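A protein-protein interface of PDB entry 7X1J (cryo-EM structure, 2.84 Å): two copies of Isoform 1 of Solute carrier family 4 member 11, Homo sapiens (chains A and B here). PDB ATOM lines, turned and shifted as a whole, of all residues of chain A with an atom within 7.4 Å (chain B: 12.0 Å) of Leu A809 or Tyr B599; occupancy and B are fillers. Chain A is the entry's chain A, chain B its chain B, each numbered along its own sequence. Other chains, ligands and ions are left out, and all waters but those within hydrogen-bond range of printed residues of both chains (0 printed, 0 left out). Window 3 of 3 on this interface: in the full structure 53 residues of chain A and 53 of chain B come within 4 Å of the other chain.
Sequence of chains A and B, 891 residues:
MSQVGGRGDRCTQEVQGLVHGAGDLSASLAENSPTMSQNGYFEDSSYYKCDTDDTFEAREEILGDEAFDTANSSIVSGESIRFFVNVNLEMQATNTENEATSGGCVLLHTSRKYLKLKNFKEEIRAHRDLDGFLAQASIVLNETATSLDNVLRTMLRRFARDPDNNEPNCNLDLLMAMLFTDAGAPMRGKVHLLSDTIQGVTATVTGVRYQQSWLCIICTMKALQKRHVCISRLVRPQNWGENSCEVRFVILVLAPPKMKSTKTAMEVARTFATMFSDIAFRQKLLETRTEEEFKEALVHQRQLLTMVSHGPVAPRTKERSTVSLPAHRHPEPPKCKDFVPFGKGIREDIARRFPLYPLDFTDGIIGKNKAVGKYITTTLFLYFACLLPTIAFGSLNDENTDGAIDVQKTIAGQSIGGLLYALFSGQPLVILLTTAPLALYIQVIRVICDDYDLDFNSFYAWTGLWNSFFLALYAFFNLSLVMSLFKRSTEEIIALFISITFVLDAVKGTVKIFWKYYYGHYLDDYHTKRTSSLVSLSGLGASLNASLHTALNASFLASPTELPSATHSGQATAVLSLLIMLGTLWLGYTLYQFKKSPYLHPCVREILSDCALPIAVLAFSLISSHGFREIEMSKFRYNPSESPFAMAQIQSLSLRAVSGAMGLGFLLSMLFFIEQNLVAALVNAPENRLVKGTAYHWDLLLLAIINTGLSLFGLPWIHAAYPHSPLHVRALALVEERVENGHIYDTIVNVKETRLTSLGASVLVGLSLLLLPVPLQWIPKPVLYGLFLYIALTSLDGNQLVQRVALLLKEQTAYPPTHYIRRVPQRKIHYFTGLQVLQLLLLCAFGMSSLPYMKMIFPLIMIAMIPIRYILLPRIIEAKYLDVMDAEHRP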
ATOM      1  N   GLN A 803      -2.418 -13.490  26.522  1.00  0.00           N
ATOM      2  CA  GLN A 803      -1.690 -13.943  27.704  1.00  0.00           C
ATOM      3  C   GLN A 803      -2.310 -15.207  28.285  1.00  0.00           C
ATOM      4  O   GLN A 803      -1.593 -16.132  28.685  1.00  0.00           O
ATOM      5  CB  GLN A 803      -1.649 -12.833  28.754  1.00  0.00           C
ATOM      6  CG  GLN A 803      -0.832 -11.620  28.344  1.00  0.00           C
ATOM      7  CD  GLN A 803      -0.887 -10.506  29.371  1.00  0.00           C
ATOM      8  OE1 GLN A 803      -1.618 -10.593  30.357  1.00  0.00           O
ATOM      9  NE2 GLN A 803      -0.112  -9.453  29.142  1.00  0.00           N
ATOM     10  N   ARG A 804      -3.642 -15.265  28.346  1.00  0.00           N
ATOM     11  CA  ARG A 804      -4.302 -16.459  28.868  1.00  0.00           C
ATOM     12  C   ARG A 804      -4.144 -17.641  27.920  1.00  0.00           C
ATOM     13  O   ARG A 804      -4.058 -18.792  28.366  1.00  0.00           O
ATOM     14  CB  ARG A 804      -5.777 -16.168  29.141  1.00  0.00           C
ATOM     15  CG  ARG A 804      -6.019 -15.492  30.484  1.00  0.00           C
ATOM     16  CD  ARG A 804      -7.498 -15.249  30.745  1.00  0.00           C
ATOM     17  NE  ARG A 804      -8.001 -14.083  30.028  1.00  0.00           N
ATOM     18  CZ  ARG A 804      -8.653 -14.135  28.876  1.00  0.00           C
ATOM     19  NH1 ARG A 804      -8.907 -15.288  28.275  1.00  0.00           N
ATOM     20  NH2 ARG A 804      -9.064 -13.004  28.313  1.00  0.00           N
ATOM     21  N   VAL A 805      -4.114 -17.384  26.610  1.00  0.00           N
ATOM     22  CA  VAL A 805      -3.835 -18.456  25.656  1.00  0.00           C
ATOM     23  C   VAL A 805      -2.433 -19.011  25.878  1.00  0.00           C
ATOM     24  O   VAL A 805      -2.229 -20.231  25.904  1.00  0.00           O
ATOM     25  CB  VAL A 805      -4.028 -17.954  24.211  1.00  0.00           C
ATOM     26  CG1 VAL A 805      -3.407 -18.928  23.222  1.00  0.00           C
ATOM     27  CG2 VAL A 805      -5.507 -17.771  23.910  1.00  0.00           C
ATOM     28  N   ALA A 806      -1.448 -18.125  26.049  1.00  0.00           N
ATOM     29  CA  ALA A 806      -0.100 -18.574  26.383  1.00  0.00           C
ATOM     30  C   ALA A 806      -0.059 -19.241  27.751  1.00  0.00           C
ATOM     31  O   ALA A 806       0.770 -20.127  27.986  1.00  0.00           O
ATOM     32  CB  ALA A 806       0.875 -17.398  26.332  1.00  0.00           C
ATOM     33  N   LEU A 807      -0.937 -18.820  28.667  1.00  0.00           N
ATOM     34  CA  LEU A 807      -1.000 -19.448  29.983  1.00  0.00           C
ATOM     35  C   LEU A 807      -1.390 -20.917  29.885  1.00  0.00           C
ATOM     36  O   LEU A 807      -0.981 -21.725  30.727  1.00  0.00           O
ATOM     37  CB  LEU A 807      -1.988 -18.690  30.872  1.00  0.00           C
ATOM     38  CG  LEU A 807      -2.002 -19.047  32.358  1.00  0.00           C
ATOM     39  CD1 LEU A 807      -0.653 -18.736  32.990  1.00  0.00           C
ATOM     40  CD2 LEU A 807      -3.119 -18.307  33.076  1.00  0.00           C
ATOM     41  N   LEU A 808      -2.314 -21.241  28.983  1.00  0.00           N
ATOM     42  CA  LEU A 808      -2.802 -22.612  28.868  1.00  0.00           C
ATOM     43  C   LEU A 808      -1.592 -23.452  28.706  1.00  0.00           C
ATOM     44  O   LEU A 808      -1.398 -24.435  29.418  1.00  0.00           O
ATOM     45  CB  LEU A 808      -3.679 -22.773  27.633  1.00  0.00           C
ATOM     46  CG  LEU A 808      -5.026 -22.064  27.572  1.00  0.00           C
ATOM     47  CD1 LEU A 808      -5.543 -22.065  26.146  1.00  0.00           C
ATOM     48  CD2 LEU A 808      -6.012 -22.745  28.498  1.00  0.00           C
ATOM     49  N   LEU A 809      -0.769 -23.078  27.745  1.00  0.00           N
ATOM     50  CA  LEU A 809       0.473 -23.778  27.554  1.00  0.00           C
ATOM     51  C   LEU A 809       1.486 -23.127  28.451  1.00  0.00           C
ATOM     52  O   LEU A 809       2.293 -22.351  27.957  1.00  0.00           O
ATOM     53  CB  LEU A 809       0.932 -23.637  26.106  1.00  0.00           C
ATOM     54  CG  LEU A 809      -0.125 -23.903  25.038  1.00  0.00           C
ATOM     55  CD1 LEU A 809       0.336 -23.365  23.694  1.00  0.00           C
ATOM     56  CD2 LEU A 809      -0.452 -25.386  24.957  1.00  0.00           C
ATOM     57  N   LYS A 810       1.448 -23.384  29.757  1.00  0.00           N
ATOM     58  CA  LYS A 810       2.479 -22.885  30.671  1.00  0.00           C
ATOM     59  C   LYS A 810       2.569 -23.865  31.823  1.00  0.00           C
ATOM     60  O   LYS A 810       1.561 -24.442  32.216  1.00  0.00           O
ATOM     61  CB  LYS A 810       2.194 -21.466  31.149  1.00  0.00           C
ATOM     62  CG  LYS A 810       3.367 -20.774  31.811  1.00  0.00           C
ATOM     63  CD  LYS A 810       3.134 -19.278  31.884  1.00  0.00           C
ATOM     64  CE  LYS A 810       3.013 -18.685  30.494  1.00  0.00           C
ATOM     65  NZ  LYS A 810       2.753 -17.221  30.545  1.00  0.00           N
ATOM     66  N   GLU A 811       3.760 -24.065  32.373  1.00  0.00           N
ATOM     67  CA  GLU A 811       3.906 -24.935  33.531  1.00  0.00           C
ATOM     68  C   GLU A 811       3.290 -24.243  34.726  1.00  0.00           C
ATOM     69  O   GLU A 811       3.347 -23.024  34.830  1.00  0.00           O
ATOM     70  CB  GLU A 811       5.368 -25.311  33.776  1.00  0.00           C
ATOM     71  CG  GLU A 811       6.278 -24.157  34.147  1.00  0.00           C
ATOM     72  CD  GLU A 811       7.740 -24.545  34.138  1.00  0.00           C
ATOM     73  OE1 GLU A 811       8.051 -25.661  33.679  1.00  0.00           O
ATOM     74  OE2 GLU A 811       8.576 -23.731  34.583  1.00  0.00           O
ATOM     75  N   ALA A 814       5.113 -21.541  36.642  1.00  0.00           N
ATOM     76  CA  ALA A 814       5.396 -20.293  35.947  1.00  0.00           C
ATOM     77  C   ALA A 814       4.193 -19.360  35.881  1.00  0.00           C
ATOM     78  O   ALA A 814       4.272 -18.315  35.228  1.00  0.00           O
ATOM     79  CB  ALA A 814       5.909 -20.580  34.534  1.00  0.00           C
ATOM     80  N   TYR A 815       3.089 -19.710  36.528  1.00  0.00           N
ATOM     81  CA  TYR A 815       1.897 -18.865  36.505  1.00  0.00           C
ATOM     82  C   TYR A 815       2.155 -17.564  37.252  1.00  0.00           C
ATOM     83  O   TYR A 815       2.521 -17.601  38.435  1.00  0.00           O
ATOM     84  CB  TYR A 815       0.713 -19.603  37.124  1.00  0.00           C
ATOM     85  CG  TYR A 815      -0.039 -20.489  36.157  1.00  0.00           C
ATOM     86  CD1 TYR A 815       0.631 -21.410  35.365  1.00  0.00           C
ATOM     87  CD2 TYR A 815      -1.421 -20.414  36.046  1.00  0.00           C
ATOM     88  CE1 TYR A 815      -0.050 -22.224  34.481  1.00  0.00           C
ATOM     89  CE2 TYR A 815      -2.113 -21.226  35.166  1.00  0.00           C
ATOM     90  CZ  TYR A 815      -1.422 -22.128  34.386  1.00  0.00           C
ATOM     91  OH  TYR A 815      -2.101 -22.940  33.508  1.00  0.00           O
ATOM     92  N   HIS A 830      -9.607 -21.025  32.244  1.00  0.00           N
ATOM     93  CA  HIS A 830      -9.369 -21.743  30.996  1.00  0.00           C
ATOM     94  C   HIS A 830     -10.664 -21.941  30.217  1.00  0.00           C
ATOM     95  O   HIS A 830     -10.663 -21.891  28.981  1.00  0.00           O
ATOM     96  CB  HIS A 830      -8.692 -23.082  31.284  1.00  0.00           C
ATOM     97  CG  HIS A 830      -7.294 -22.948  31.803  1.00  0.00           C
ATOM     98  ND1 HIS A 830      -6.645 -21.735  31.885  1.00  0.00           N
ATOM     99  CD2 HIS A 830      -6.418 -23.874  32.260  1.00  0.00           C
ATOM    100  CE1 HIS A 830      -5.431 -21.919  32.372  1.00  0.00           C
ATOM    101  NE2 HIS A 830      -5.268 -23.208  32.609  1.00  0.00           N
ATOM    102  N   THR B 590      16.279 -20.724  18.262  1.00  0.00           N
ATOM    103  CA  THR B 590      15.014 -20.549  18.970  1.00  0.00           C
ATOM    104  C   THR B 590      14.684 -21.777  19.810  1.00  0.00           C
ATOM    105  O   THR B 590      14.258 -21.661  20.966  1.00  0.00           O
ATOM    106  CB  THR B 590      13.891 -20.257  17.976  1.00  0.00           C
ATOM    107  OG1 THR B 590      14.208 -19.080  17.224  1.00  0.00           O
ATOM    108  CG2 THR B 590      12.571 -20.043  18.704  1.00  0.00           C
ATOM    109  N   LEU B 591      14.871 -22.969  19.239  1.00  0.00           N
ATOM    110  CA  LEU B 591      14.662 -24.193  20.005  1.00  0.00           C
ATOM    111  C   LEU B 591      15.711 -24.344  21.099  1.00  0.00           C
ATOM    112  O   LEU B 591      15.422 -24.883  22.172  1.00  0.00           O
ATOM    113  CB  LEU B 591      14.675 -25.406  19.074  1.00  0.00           C
ATOM    114  CG  LEU B 591      13.527 -25.511  18.069  1.00  0.00           C
ATOM    115  CD1 LEU B 591      13.705 -26.732  17.178  1.00  0.00           C
ATOM    116  CD2 LEU B 591      12.187 -25.563  18.786  1.00  0.00           C
ATOM    117  N   TYR B 592      16.938 -23.882  20.841  1.00  0.00           N
ATOM    118  CA  TYR B 592      17.983 -23.944  21.857  1.00  0.00           C
ATOM    119  C   TYR B 592      17.617 -23.112  23.079  1.00  0.00           C
ATOM    120  O   TYR B 592      17.822 -23.544  24.219  1.00  0.00           O
ATOM    121  CB  TYR B 592      19.314 -23.477  21.265  1.00  0.00           C
ATOM    122  CG  TYR B 592      20.397 -23.246  22.295  1.00  0.00           C
ATOM    123  CD1 TYR B 592      21.091 -24.310  22.853  1.00  0.00           C
ATOM    124  CD2 TYR B 592      20.729 -21.959  22.702  1.00  0.00           C
ATOM    125  CE1 TYR B 592      22.084 -24.101  23.791  1.00  0.00           C
ATOM    126  CE2 TYR B 592      21.719 -21.741  23.640  1.00  0.00           C
ATOM    127  CZ  TYR B 592      22.393 -22.815  24.182  1.00  0.00           C
ATOM    128  OH  TYR B 592      23.380 -22.600  25.116  1.00  0.00           O
ATOM    129  N   GLN B 593      17.073 -21.914  22.863  1.00  0.00           N
ATOM    130  CA  GLN B 593      16.651 -21.059  23.963  1.00  0.00           C
ATOM    131  C   GLN B 593      15.292 -21.446  24.529  1.00  0.00           C
ATOM    132  O   GLN B 593      14.873 -20.869  25.539  1.00  0.00           O
ATOM    133  CB  GLN B 593      16.618 -19.598  23.514  1.00  0.00           C
ATOM    134  CG  GLN B 593      17.987 -18.997  23.253  1.00  0.00           C
ATOM    135  CD  GLN B 593      17.909 -17.554  22.795  1.00  0.00           C
ATOM    136  OE1 GLN B 593      16.950 -17.151  22.135  1.00  0.00           O
ATOM    137  NE2 GLN B 593      18.920 -16.767  23.142  1.00  0.00           N
ATOM    138  N   PHE B 594      14.594 -22.400  23.907  1.00  0.00           N
ATOM    139  CA  PHE B 594      13.288 -22.817  24.402  1.00  0.00           C
ATOM    140  C   PHE B 594      13.372 -23.508  25.757  1.00  0.00           C
ATOM    141  O   PHE B 594      12.357 -23.594  26.456  1.00  0.00           O
ATOM    142  CB  PHE B 594      12.618 -23.740  23.378  1.00  0.00           C
ATOM    143  CG  PHE B 594      11.212 -24.135  23.738  1.00  0.00           C
ATOM    144  CD1 PHE B 594      10.173 -23.225  23.631  1.00  0.00           C
ATOM    145  CD2 PHE B 594      10.930 -25.420  24.172  1.00  0.00           C
ATOM    146  CE1 PHE B 594       8.879 -23.589  23.958  1.00  0.00           C
ATOM    147  CE2 PHE B 594       9.638 -25.789  24.498  1.00  0.00           C
ATOM    148  CZ  PHE B 594       8.611 -24.872  24.392  1.00  0.00           C
ATOM    149  N   LYS B 595      14.555 -23.990  26.148  1.00  0.00           N
ATOM    150  CA  LYS B 595      14.701 -24.683  27.425  1.00  0.00           C
ATOM    151  C   LYS B 595      14.455 -23.769  28.617  1.00  0.00           C
ATOM    152  O   LYS B 595      14.090 -24.259  29.692  1.00  0.00           O
ATOM    153  CB  LYS B 595      16.094 -25.308  27.529  1.00  0.00           C
ATOM    154  CG  LYS B 595      17.235 -24.308  27.431  1.00  0.00           C
ATOM    155  CD  LYS B 595      18.587 -25.000  27.496  1.00  0.00           C
ATOM    156  CE  LYS B 595      19.727 -23.997  27.414  1.00  0.00           C
ATOM    157  NZ  LYS B 595      19.694 -23.213  26.146  1.00  0.00           N
ATOM    158  N   LYS B 596      14.677 -22.474  28.453  1.00  0.00           N
ATOM    159  CA  LYS B 596      14.522 -21.543  29.557  1.00  0.00           C
ATOM    160  C   LYS B 596      13.104 -21.030  29.609  1.00  0.00           C
ATOM    161  O   LYS B 596      12.727 -20.325  30.541  1.00  0.00           O
ATOM    162  CB  LYS B 596      15.493 -20.379  29.386  1.00  0.00           C
ATOM    163  CG  LYS B 596      16.955 -20.791  29.361  1.00  0.00           C
ATOM    164  CD  LYS B 596      17.344 -21.496  30.651  1.00  0.00           C
ATOM    165  CE  LYS B 596      18.799 -21.932  30.628  1.00  0.00           C
ATOM    166  NZ  LYS B 596      19.190 -22.623  31.886  1.00  0.00           N
ATOM    167  N   SER B 597      12.311 -21.379  28.608  1.00  0.00           N
ATOM    168  CA  SER B 597      10.943 -20.900  28.543  1.00  0.00           C
ATOM    169  C   SER B 597      10.027 -21.517  29.576  1.00  0.00           C
ATOM    170  O   SER B 597      10.206 -22.665  29.959  1.00  0.00           O
ATOM    171  CB  SER B 597      10.366 -21.131  27.148  1.00  0.00           C
ATOM    172  OG  SER B 597       9.885 -22.454  27.014  1.00  0.00           O
ATOM    173  N   PRO B 598       8.991 -20.766  30.029  1.00  0.00           N
ATOM    174  CA  PRO B 598       8.095 -21.452  30.964  1.00  0.00           C
ATOM    175  C   PRO B 598       7.131 -22.371  30.253  1.00  0.00           C
ATOM    176  O   PRO B 598       6.378 -23.083  30.904  1.00  0.00           O
ATOM    177  CB  PRO B 598       7.307 -20.299  31.555  1.00  0.00           C
ATOM    178  CG  PRO B 598       7.227 -19.299  30.467  1.00  0.00           C
ATOM    179  CD  PRO B 598       8.602 -19.338  29.888  1.00  0.00           C
ATOM    180  N   TYR B 599       7.140 -22.357  28.931  1.00  0.00           N
ATOM    181  CA  TYR B 599       6.178 -23.137  28.169  1.00  0.00           C
ATOM    182  C   TYR B 599       6.373 -24.639  28.145  1.00  0.00           C
ATOM    183  O   TYR B 599       7.511 -25.092  28.128  1.00  0.00           O
ATOM    184  CB  TYR B 599       6.097 -22.584  26.747  1.00  0.00           C
ATOM    185  CG  TYR B 599       5.907 -21.083  26.702  1.00  0.00           C
ATOM    186  CD1 TYR B 599       4.710 -20.504  27.089  1.00  0.00           C
ATOM    187  CD2 TYR B 599       6.926 -20.249  26.272  1.00  0.00           C
ATOM    188  CE1 TYR B 599       4.530 -19.138  27.054  1.00  0.00           C
ATOM    189  CE2 TYR B 599       6.757 -18.879  26.234  1.00  0.00           C
ATOM    190  CZ  TYR B 599       5.556 -18.331  26.626  1.00  0.00           C
ATOM    191  OH  TYR B 599       5.380 -16.968  26.590  1.00  0.00           O
ATOM    192  N   LEU B 600       5.281 -25.401  28.186  1.00  0.00           N
ATOM    193  CA  LEU B 600       5.320 -26.874  28.092  1.00  0.00           C
ATOM    194  C   LEU B 600       5.686 -27.639  29.353  1.00  0.00           C
ATOM    195  O   LEU B 600       5.967 -27.042  30.389  1.00  0.00           O
ATOM    196  CB  LEU B 600       6.121 -27.379  26.879  1.00  0.00           C
ATOM    197  CG  LEU B 600       5.412 -27.575  25.537  1.00  0.00           C
ATOM    198  CD1 LEU B 600       4.820 -26.282  25.000  1.00  0.00           C
ATOM    199  CD2 LEU B 600       6.372 -28.182  24.528  1.00  0.00           C
ATOM    200  N   HIS B 601       5.690 -28.962  29.261  1.00  0.00           N
ATOM    201  CA  HIS B 601       6.059 -29.785  30.402  1.00  0.00           C
ATOM    202  C   HIS B 601       7.583 -29.738  30.533  1.00  0.00           C
ATOM    203  O   HIS B 601       8.264 -29.748  29.521  1.00  0.00           O
ATOM    204  CB  HIS B 601       5.570 -31.218  30.225  1.00  0.00           C
ATOM    205  CG  HIS B 601       5.717 -32.061  31.450  1.00  0.00           C
ATOM    206  ND1 HIS B 601       6.732 -32.980  31.604  1.00  0.00           N
ATOM    207  CD2 HIS B 601       4.986 -32.112  32.588  1.00  0.00           C
ATOM    208  CE1 HIS B 601       6.615 -33.567  32.781  1.00  0.00           C
ATOM    209  NE2 HIS B 601       5.566 -33.058  33.398  1.00  0.00           N
ATOM    210  N   PRO B 602       8.135 -29.689  31.773  1.00  0.00           N
ATOM    211  CA  PRO B 602       9.591 -29.553  31.801  1.00  0.00           C
ATOM    212  C   PRO B 602      10.305 -30.653  31.035  1.00  0.00           C
ATOM    213  O   PRO B 602      11.284 -30.367  30.356  1.00  0.00           O
ATOM    214  CB  PRO B 602       9.915 -29.667  33.287  1.00  0.00           C
ATOM    215  CG  PRO B 602       8.701 -29.155  33.977  1.00  0.00           C
ATOM    216  CD  PRO B 602       7.531 -29.509  33.105  1.00  0.00           C
ATOM    217  N   CYS B 603       9.837 -31.887  31.145  1.00  0.00           N
ATOM    218  CA  CYS B 603      10.458 -32.996  30.440  1.00  0.00           C
ATOM    219  C   CYS B 603      10.316 -32.844  28.938  1.00  0.00           C
ATOM    220  O   CYS B 603      11.297 -32.949  28.213  1.00  0.00           O
ATOM    221  CB  CYS B 603       9.852 -34.321  30.888  1.00  0.00           C
ATOM    222  SG  CYS B 603      10.092 -34.678  32.642  1.00  0.00           S
ATOM    223  N   VAL B 604       9.099 -32.599  28.469  1.00  0.00           N
ATOM    224  CA  VAL B 604       8.885 -32.422  27.036  1.00  0.00           C
ATOM    225  C   VAL B 604       9.689 -31.238  26.512  1.00  0.00           C
ATOM    226  O   VAL B 604      10.277 -31.302  25.426  1.00  0.00           O
ATOM    227  CB  VAL B 604       7.382 -32.265  26.744  1.00  0.00           C
ATOM    228  CG1 VAL B 604       7.143 -32.076  25.254  1.00  0.00           C
ATOM    229  CG2 VAL B 604       6.609 -33.470  27.270  1.00  0.00           C
ATOM    230  N   ARG B 605       9.729 -30.138  27.273  1.00  0.00           N
ATOM    231  CA  ARG B 605      10.471 -28.963  26.830  1.00  0.00           C
ATOM    232  C   ARG B 605      11.965 -29.246  26.740  1.00  0.00           C
ATOM    233  O   ARG B 605      12.626 -28.817  25.786  1.00  0.00           O
ATOM    234  CB  ARG B 605      10.208 -27.789  27.771  1.00  0.00           C
ATOM    235  CG  ARG B 605      11.138 -26.612  27.558  1.00  0.00           C
ATOM    236  CD  ARG B 605      10.786 -25.461  28.474  1.00  0.00           C
ATOM    237  NE  ARG B 605      11.002 -25.778  29.882  1.00  0.00           N
ATOM    238  CZ  ARG B 605      10.034 -26.022  30.753  1.00  0.00           C
ATOM    239  NH1 ARG B 605       8.760 -25.989  30.399  1.00  0.00           N
ATOM    240  NH2 ARG B 605      10.353 -26.300  32.014  1.00  0.00           N
ATOM    241  N   GLU B 606      12.518 -29.954  27.728  1.00  0.00           N
ATOM    242  CA  GLU B 606      13.945 -30.259  27.708  1.00  0.00           C
ATOM    243  C   GLU B 606      14.305 -31.136  26.517  1.00  0.00           C
ATOM    244  O   GLU B 606      15.324 -30.909  25.855  1.00  0.00           O
ATOM    245  CB  GLU B 606      14.355 -30.931  29.018  1.00  0.00           C
ATOM    246  CG  GLU B 606      15.841 -31.225  29.128  1.00  0.00           C
ATOM    247  CD  GLU B 606      16.205 -31.864  30.452  1.00  0.00           C
ATOM    248  OE1 GLU B 606      15.293 -32.092  31.273  1.00  0.00           O
ATOM    249  OE2 GLU B 606      17.404 -32.137  30.674  1.00  0.00           O
ATOM    250  N   ILE B 607      13.480 -32.144  26.228  1.00  0.00           N
ATOM    251  CA  ILE B 607      13.730 -33.002  25.074  1.00  0.00           C
ATOM    252  C   ILE B 607      13.612 -32.207  23.779  1.00  0.00           C
ATOM    253  O   ILE B 607      14.451 -32.335  22.878  1.00  0.00           O
ATOM    254  CB  ILE B 607      12.774 -34.208  25.090  1.00  0.00           C
ATOM    255  CG1 ILE B 607      13.082 -35.116  26.283  1.00  0.00           C
ATOM    256  CG2 ILE B 607      12.868 -34.987  23.787  1.00  0.00           C
ATOM    257  CD1 ILE B 607      12.153 -36.304  26.401  1.00  0.00           C
ATOM    258  N   LEU B 608      12.575 -31.374  23.663  1.00  0.00           N
ATOM    259  CA  LEU B 608      12.390 -30.588  22.446  1.00  0.00           C
ATOM    260  C   LEU B 608      13.520 -29.581  22.259  1.00  0.00           C
ATOM    261  O   LEU B 608      14.003 -29.381  21.138  1.00  0.00           O
ATOM    262  CB  LEU B 608      11.036 -29.877  22.482  1.00  0.00           C
ATOM    263  CG  LEU B 608      10.605 -29.177  21.192  1.00  0.00           C
ATOM    264  CD1 LEU B 608      10.422 -30.188  20.068  1.00  0.00           C
ATOM    265  CD2 LEU B 608       9.329 -28.378  21.411  1.00  0.00           C
ATOM    266  N   SER B 609      13.954 -28.937  23.345  1.00  0.00           N
ATOM    267  CA  SER B 609      15.007 -27.932  23.234  1.00  0.00           C
ATOM    268  C   SER B 609      16.359 -28.569  22.937  1.00  0.00           C
ATOM    269  O   SER B 609      17.126 -28.053  22.115  1.00  0.00           O
ATOM    270  CB  SER B 609      15.080 -27.101  24.514  1.00  0.00           C
ATOM    271  OG  SER B 609      16.096 -26.118  24.421  1.00  0.00           O
ATOM    272  N   ASP B 610      16.671 -29.687  23.598  1.00  0.00           N
ATOM    273  CA  ASP B 610      17.945 -30.358  23.360  1.00  0.00           C
ATOM    274  C   ASP B 610      18.028 -30.964  21.963  1.00  0.00           C
ATOM    275  O   ASP B 610      19.128 -31.297  21.513  1.00  0.00           O
ATOM    276  CB  ASP B 610      18.181 -31.435  24.417  1.00  0.00           C
ATOM    277  CG  ASP B 610      18.434 -30.854  25.795  1.00  0.00           C
ATOM    278  OD1 ASP B 610      18.906 -29.700  25.879  1.00  0.00           O
ATOM    279  OD2 ASP B 610      18.165 -31.552  26.795  1.00  0.00           O
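The backbone carbonyl oxygen of Leu B600 is in hydrogen-bond range of the guanidinium group of Arg B605. NE of Arg B605 sits at hydrogen-bond distance from O of Ser B597, 3.2 Å away. The backbone carbonyl oxygen (O) of Tyr B599 lies within hydrogen-bond range of the guanidinium group (NH1) of Arg B605 (2.7 Å). The backbone carbonyl oxygen (O) of Lys B595 is in hydrogen-bond range of the guanidinium group (NE) of Arg B605. OG of Ser B597 lies close to N of Tyr B599 (3.3 Å).
No position is printed for both chains. Of the 9 pairs that touch across the chains among the printed residues, none has its exchanged pair printed and touching as well.
Ala A806 touches Tyr B599 (O to CE1, 3.998 Å). O of Leu A809 touches CD1 of Tyr B599, at 3.2 Å. Pro B598 touches Lys A810 (O to CG, 3.9 Å). CE1 of Tyr B599 touches CE of Lys A810, at 3.8 Å. Glu A811 touches Leu B600 (CB to O, 3.9 Å). Glu A811 touches Pro B602. CB of Ala A814 touches CB of Pro B598 (3.3 Å).
Of chain B, only Tyr B599 comes within 4 Å of Leu A809. Printed residues of chain A within 4 Å of Tyr B599: Ala A806 (3.998 Å), Leu A809 (3.2 Å) and Lys A810 (3.8 Å). No residue of chain B comes within 4 Å of Leu A807. No residue of chain B comes within 4 Å of Leu A808. Lys A810 touches two residues of chain B. Of the printed residues of chain A, Pro B602 touches Glu A811 (3.6 Å). Of the printed residues of chain A, Arg B605 touches Glu A811 (2.9 Å). Of the printed residues of chain B, Ala A806 touches Tyr B599 (3.998 Å). The nearest printed residue of chain A that does not touch Tyr B599 is Glu A811 (4.9 Å). The nearest printed residue of chain A that does not touch Arg B605 is Lys A810 (6.7 Å).
O of Pro B598 sits at hydrogen-bond distance from N of Glu A811 (3.2 Å). OE1 of Glu A811 lies within salt-bridge range of NH2 of Arg B605 (2.9 Å).
Hydrophobic or aromatic side chains of chain A that line the printed part of chain B: Ala A814. Of the 21 printed residues of chain B, 5 touch a printed residue of chain A. Hydrophobic or aromatic side chains of chain B within 4 Å of the printed part of chain A: Pro B598, Tyr B599 and Pro B602. Among the printed residues, 9 pairs touch across the chains.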
